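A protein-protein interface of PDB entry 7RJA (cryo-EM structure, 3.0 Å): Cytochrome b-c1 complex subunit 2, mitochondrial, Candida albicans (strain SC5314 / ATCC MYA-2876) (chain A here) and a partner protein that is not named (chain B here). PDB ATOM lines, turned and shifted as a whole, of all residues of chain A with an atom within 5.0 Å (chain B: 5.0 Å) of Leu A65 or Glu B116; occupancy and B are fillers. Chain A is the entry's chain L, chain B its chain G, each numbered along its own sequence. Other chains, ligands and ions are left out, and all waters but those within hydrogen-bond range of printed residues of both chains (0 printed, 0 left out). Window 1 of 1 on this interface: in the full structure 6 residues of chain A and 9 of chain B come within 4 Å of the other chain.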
ATOM      1  N   SER A  63     -12.215  -6.743   0.095  1.00  0.00           N
ATOM      2  CA  SER A  63     -12.594  -5.617   0.932  1.00  0.00           C
ATOM      3  C   SER A  63     -11.729  -4.405   0.600  1.00  0.00           C
ATOM      4  O   SER A  63     -10.874  -4.437  -0.286  1.00  0.00           O
ATOM      5  CB  SER A  63     -12.463  -5.992   2.404  1.00  0.00           C
ATOM      6  OG  SER A  63     -11.116  -6.274   2.731  1.00  0.00           O
ATOM      7  N   ALA A  64     -11.969  -3.306   1.316  1.00  0.00           N
ATOM      8  CA  ALA A  64     -11.148  -2.116   1.131  1.00  0.00           C
ATOM      9  C   ALA A  64      -9.722  -2.361   1.590  1.00  0.00           C
ATOM     10  O   ALA A  64      -8.764  -2.082   0.862  1.00  0.00           O
ATOM     11  CB  ALA A  64     -11.750  -0.939   1.895  1.00  0.00           C
ATOM     12  N   LEU A  65      -9.560  -2.888   2.800  1.00  0.00           N
ATOM     13  CA  LEU A  65      -8.233  -3.060   3.361  1.00  0.00           C
ATOM     14  C   LEU A  65      -7.412  -4.088   2.604  1.00  0.00           C
ATOM     15  O   LEU A  65      -6.188  -4.106   2.754  1.00  0.00           O
ATOM     16  CB  LEU A  65      -8.352  -3.445   4.833  1.00  0.00           C
ATOM     17  CG  LEU A  65      -7.063  -3.404   5.641  1.00  0.00           C
ATOM     18  CD1 LEU A  65      -7.336  -2.906   7.043  1.00  0.00           C
ATOM     19  CD2 LEU A  65      -6.450  -4.777   5.696  1.00  0.00           C
ATOM     20  N   ARG A  66      -8.045  -4.940   1.801  1.00  0.00           N
ATOM     21  CA  ARG A  66      -7.306  -5.887   0.979  1.00  0.00           C
ATOM     22  C   ARG A  66      -7.015  -5.315  -0.399  1.00  0.00           C
ATOM     23  O   ARG A  66      -5.877  -5.379  -0.872  1.00  0.00           O
ATOM     24  CB  ARG A  66      -8.081  -7.197   0.848  1.00  0.00           C
ATOM     25  CG  ARG A  66      -7.394  -8.217  -0.037  1.00  0.00           C
ATOM     26  CD  ARG A  66      -7.950  -9.610   0.174  1.00  0.00           C
ATOM     27  NE  ARG A  66      -7.546 -10.163   1.460  1.00  0.00           N
ATOM     28  CZ  ARG A  66      -6.339 -10.642   1.726  1.00  0.00           C
ATOM     29  NH1 ARG A  66      -5.381 -10.646   0.815  1.00  0.00           N
ATOM     30  NH2 ARG A  66      -6.085 -11.126   2.938  1.00  0.00           N
ATOM     31  N   PHE A  67      -8.030  -4.758  -1.059  1.00  0.00           N
ATOM     32  CA  PHE A  67      -7.813  -4.227  -2.396  1.00  0.00           C
ATOM     33  C   PHE A  67      -6.848  -3.054  -2.376  1.00  0.00           C
ATOM     34  O   PHE A  67      -5.972  -2.968  -3.238  1.00  0.00           O
ATOM     35  CB  PHE A  67      -9.134  -3.802  -3.027  1.00  0.00           C
ATOM     36  CG  PHE A  67      -8.968  -2.864  -4.184  1.00  0.00           C
ATOM     37  CD1 PHE A  67      -8.512  -3.329  -5.402  1.00  0.00           C
ATOM     38  CD2 PHE A  67      -9.267  -1.524  -4.059  1.00  0.00           C
ATOM     39  CE1 PHE A  67      -8.356  -2.477  -6.470  1.00  0.00           C
ATOM     40  CE2 PHE A  67      -9.112  -0.666  -5.128  1.00  0.00           C
ATOM     41  CZ  PHE A  67      -8.656  -1.146  -6.334  1.00  0.00           C
ATOM     42  N   THR A  68      -6.980  -2.146  -1.408  1.00  0.00           N
ATOM     43  CA  THR A  68      -6.058  -1.020  -1.321  1.00  0.00           C
ATOM     44  C   THR A  68      -4.632  -1.482  -1.060  1.00  0.00           C
ATOM     45  O   THR A  68      -3.693  -0.992  -1.695  1.00  0.00           O
ATOM     46  CB  THR A  68      -6.496  -0.059  -0.220  1.00  0.00           C
ATOM     47  OG1 THR A  68      -7.857   0.332  -0.433  1.00  0.00           O
ATOM     48  CG2 THR A  68      -5.613   1.168  -0.205  1.00  0.00           C
ATOM     49  N   ARG A  69      -4.450  -2.418  -0.130  1.00  0.00           N
ATOM     50  CA  ARG A  69      -3.110  -2.909   0.165  1.00  0.00           C
ATOM     51  C   ARG A  69      -2.493  -3.576  -1.054  1.00  0.00           C
ATOM     52  O   ARG A  69      -1.328  -3.332  -1.384  1.00  0.00           O
ATOM     53  CB  ARG A  69      -3.159  -3.884   1.338  1.00  0.00           C
ATOM     54  CG  ARG A  69      -3.451  -3.237   2.673  1.00  0.00           C
ATOM     55  CD  ARG A  69      -2.315  -2.359   3.131  1.00  0.00           C
ATOM     56  NE  ARG A  69      -1.978  -2.613   4.524  1.00  0.00           N
ATOM     57  CZ  ARG A  69      -2.620  -2.092   5.559  1.00  0.00           C
ATOM     58  NH1 ARG A  69      -3.663  -1.296   5.396  1.00  0.00           N
ATOM     59  NH2 ARG A  69      -2.207  -2.378   6.789  1.00  0.00           N
ATOM     60  N   GLU B 111     -13.857  -8.247  13.626  1.00  0.00           N
ATOM     61  CA  GLU B 111     -12.758  -9.199  13.684  1.00  0.00           C
ATOM     62  C   GLU B 111     -12.248  -9.545  12.295  1.00  0.00           C
ATOM     63  O   GLU B 111     -11.051  -9.771  12.125  1.00  0.00           O
ATOM     64  CB  GLU B 111     -13.190 -10.459  14.423  1.00  0.00           C
ATOM     65  CG  GLU B 111     -13.463 -10.231  15.893  1.00  0.00           C
ATOM     66  CD  GLU B 111     -13.904 -11.490  16.599  1.00  0.00           C
ATOM     67  OE1 GLU B 111     -14.116 -12.510  15.909  1.00  0.00           O
ATOM     68  OE2 GLU B 111     -14.033 -11.465  17.840  1.00  0.00           O
ATOM     69  N   LYS B 112     -13.128  -9.604  11.296  1.00  0.00           N
ATOM     70  CA  LYS B 112     -12.677  -9.823   9.928  1.00  0.00           C
ATOM     71  C   LYS B 112     -11.755  -8.698   9.483  1.00  0.00           C
ATOM     72  O   LYS B 112     -10.693  -8.943   8.900  1.00  0.00           O
ATOM     73  CB  LYS B 112     -13.881  -9.929   8.994  1.00  0.00           C
ATOM     74  CG  LYS B 112     -13.527 -10.269   7.555  1.00  0.00           C
ATOM     75  CD  LYS B 112     -14.761 -10.307   6.660  1.00  0.00           C
ATOM     76  CE  LYS B 112     -15.627 -11.527   6.922  1.00  0.00           C
ATOM     77  NZ  LYS B 112     -14.953 -12.790   6.516  1.00  0.00           N
ATOM     78  N   GLU B 113     -12.142  -7.454   9.760  1.00  0.00           N
ATOM     79  CA  GLU B 113     -11.295  -6.323   9.399  1.00  0.00           C
ATOM     80  C   GLU B 113      -9.954  -6.397  10.117  1.00  0.00           C
ATOM     81  O   GLU B 113      -8.894  -6.216   9.505  1.00  0.00           O
ATOM     82  CB  GLU B 113     -12.002  -5.012   9.729  1.00  0.00           C
ATOM     83  CG  GLU B 113     -13.131  -4.663   8.784  1.00  0.00           C
ATOM     84  CD  GLU B 113     -14.002  -3.545   9.313  1.00  0.00           C
ATOM     85  OE1 GLU B 113     -13.472  -2.665  10.024  1.00  0.00           O
ATOM     86  OE2 GLU B 113     -15.215  -3.546   9.023  1.00  0.00           O
ATOM     87  N   ALA B 114      -9.982  -6.672  11.422  1.00  0.00           N
ATOM     88  CA  ALA B 114      -8.741  -6.730  12.186  1.00  0.00           C
ATOM     89  C   ALA B 114      -7.846  -7.862  11.700  1.00  0.00           C
ATOM     90  O   ALA B 114      -6.625  -7.703  11.609  1.00  0.00           O
ATOM     91  CB  ALA B 114      -9.050  -6.893  13.671  1.00  0.00           C
ATOM     92  N   PHE B 115      -8.435  -9.017  11.389  1.00  0.00           N
ATOM     93  CA  PHE B 115      -7.647 -10.152  10.930  1.00  0.00           C
ATOM     94  C   PHE B 115      -7.049  -9.888   9.559  1.00  0.00           C
ATOM     95  O   PHE B 115      -5.897 -10.256   9.306  1.00  0.00           O
ATOM     96  CB  PHE B 115      -8.506 -11.415  10.904  1.00  0.00           C
ATOM     97  CG  PHE B 115      -8.839 -11.961  12.269  1.00  0.00           C
ATOM     98  CD1 PHE B 115      -8.411 -11.324  13.424  1.00  0.00           C
ATOM     99  CD2 PHE B 115      -9.584 -13.120  12.394  1.00  0.00           C
ATOM    100  CE1 PHE B 115      -8.720 -11.831  14.668  1.00  0.00           C
ATOM    101  CE2 PHE B 115      -9.896 -13.630  13.637  1.00  0.00           C
ATOM    102  CZ  PHE B 115      -9.463 -12.983  14.774  1.00  0.00           C
ATOM    103  N   GLU B 116      -7.802  -9.259   8.654  1.00  0.00           N
ATOM    104  CA  GLU B 116      -7.213  -8.903   7.369  1.00  0.00           C
ATOM    105  C   GLU B 116      -6.079  -7.908   7.547  1.00  0.00           C
ATOM    106  O   GLU B 116      -5.044  -8.013   6.881  1.00  0.00           O
ATOM    107  CB  GLU B 116      -8.264  -8.339   6.416  1.00  0.00           C
ATOM    108  CG  GLU B 116      -9.303  -9.344   5.969  1.00  0.00           C
ATOM    109  CD  GLU B 116     -10.325  -8.734   5.039  1.00  0.00           C
ATOM    110  OE1 GLU B 116     -10.290  -7.499   4.846  1.00  0.00           O
ATOM    111  OE2 GLU B 116     -11.161  -9.484   4.496  1.00  0.00           O
ATOM    112  N   LYS B 117      -6.251  -6.929   8.434  1.00  0.00           N
ATOM    113  CA  LYS B 117      -5.174  -5.970   8.655  1.00  0.00           C
ATOM    114  C   LYS B 117      -3.933  -6.661   9.202  1.00  0.00           C
ATOM    115  O   LYS B 117      -2.813  -6.387   8.757  1.00  0.00           O
ATOM    116  CB  LYS B 117      -5.633  -4.866   9.601  1.00  0.00           C
ATOM    117  CG  LYS B 117      -4.624  -3.748   9.749  1.00  0.00           C
ATOM    118  CD  LYS B 117      -5.094  -2.702  10.732  1.00  0.00           C
ATOM    119  CE  LYS B 117      -6.210  -1.860  10.149  1.00  0.00           C
ATOM    120  NZ  LYS B 117      -6.600  -0.755  11.063  1.00  0.00           N
ATOM    121  N   ALA B 118      -4.112  -7.567  10.164  1.00  0.00           N
ATOM    122  CA  ALA B 118      -2.972  -8.292  10.712  1.00  0.00           C
ATOM    123  C   ALA B 118      -2.305  -9.153   9.650  1.00  0.00           C
ATOM    124  O   ALA B 118      -1.074  -9.204   9.565  1.00  0.00           O
ATOM    125  CB  ALA B 118      -3.419  -9.154  11.891  1.00  0.00           C
ATOM    126  N   GLU B 119      -3.101  -9.841   8.832  1.00  0.00           N
ATOM    127  CA  GLU B 119      -2.534 -10.704   7.805  1.00  0.00           C
ATOM    128  C   GLU B 119      -1.754  -9.895   6.779  1.00  0.00           C
ATOM    129  O   GLU B 119      -0.665 -10.299   6.359  1.00  0.00           O
ATOM    130  CB  GLU B 119      -3.645 -11.504   7.127  1.00  0.00           C
ATOM    131  CG  GLU B 119      -3.144 -12.601   6.207  1.00  0.00           C
ATOM    132  CD  GLU B 119      -2.794 -12.096   4.824  1.00  0.00           C
ATOM    133  OE1 GLU B 119      -3.400 -11.099   4.381  1.00  0.00           O
ATOM    134  OE2 GLU B 119      -1.908 -12.695   4.178  1.00  0.00           O
ATOM    135  N   LEU B 120      -2.295  -8.749   6.362  1.00  0.00           N
ATOM    136  CA  LEU B 120      -1.621  -7.955   5.342  1.00  0.00           C
ATOM    137  C   LEU B 120      -0.390  -7.254   5.897  1.00  0.00           C
ATOM    138  O   LEU B 120       0.590  -7.064   5.168  1.00  0.00           O
ATOM    139  CB  LEU B 120      -2.591  -6.943   4.740  1.00  0.00           C
ATOM    140  CG  LEU B 120      -3.741  -7.562   3.947  1.00  0.00           C
ATOM    141  CD1 LEU B 120      -4.693  -6.492   3.486  1.00  0.00           C
ATOM    142  CD2 LEU B 120      -3.224  -8.348   2.755  1.00  0.00           C
ATOM    143  N   ASP B 121      -0.412  -6.862   7.171  1.00  0.00           N
ATOM    144  CA  ASP B 121       0.794  -6.313   7.777  1.00  0.00           C
ATOM    145  C   ASP B 121       1.921  -7.333   7.810  1.00  0.00           C
ATOM    146  O   ASP B 121       3.091  -6.944   7.884  1.00  0.00           O
ATOM    147  CB  ASP B 121       0.498  -5.822   9.193  1.00  0.00           C
ATOM    148  CG  ASP B 121      -0.159  -4.457   9.211  1.00  0.00           C
ATOM    149  OD1 ASP B 121      -0.724  -4.056   8.172  1.00  0.00           O
ATOM    150  OD2 ASP B 121      -0.110  -3.787  10.263  1.00  0.00           O
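The side-chain carboxylate (OE1) of Glu B116 sits at hydrogen-bond distance from the side-chain hydroxyl (OG) of Ser A63.
OD1 of Asp B121 lies within salt-bridge range of NH2 of Arg A69, at 2.6 Å.
The side-chain carboxylate (OE1) of Glu B119 lies within salt-bridge range of the guanidinium group (NH2) of Arg A66.
OG of Ser A63 is in hydrogen-bond range of N of Arg A66.
Printed residues of chain B within 4 Å of Ser A63: Glu B116 (2.6 Å).
Of the printed residues of chain B, Leu A65 touches Glu B116 (3.7 Å), Lys B117 (3.4 Å) and Leu B120 (2.9 Å).
Of the printed residues of chain B, Arg A66 touches Glu B119 and Leu B120.
Of chain A, only Ser A63 and Leu A65 come within 4 Å of Glu B116.
Printed residues of chain A within 4 Å of Glu B119: Arg A66.
Of the printed residues of chain A, Leu B120 touches Leu A65 (2.9 Å), Arg A66 (3.7 Å) and Arg A69 (3.6 Å).
The nearest printed residue of chain A that does not touch Leu B120 is Phe A67 (5.9 Å).
Of the 7 printed residues of chain A, 4 touch a printed residue of chain B.
Printed residues of chain A that touch a printed residue of chain B: Ser A63, Leu A65, Arg A66 and Arg A69.
Hydrophobic or aromatic side chains of chain A that line the printed part of chain B: Leu A65.
Along chain A the printed residues that touch a printed residue of chain B span positions 63 to 69.
Hydrophobic or aromatic side chains of chain B within 4 Å of the printed part of chain A: Leu B120.
Among the printed residues, 8 pairs touch across the chains.
Leu A65 touches Glu B116 (CD2 to C, 3.7 Å).
CA of Lys B117 touches CD2 of Leu A65, at 3.4 Å.
O of Leu A65 touches CD1 of Leu B120 (2.9 Å).
Arg A66 touches Leu B120 (CA to CD1, 3.7 Å).
Arg A69 touches Leu B120.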
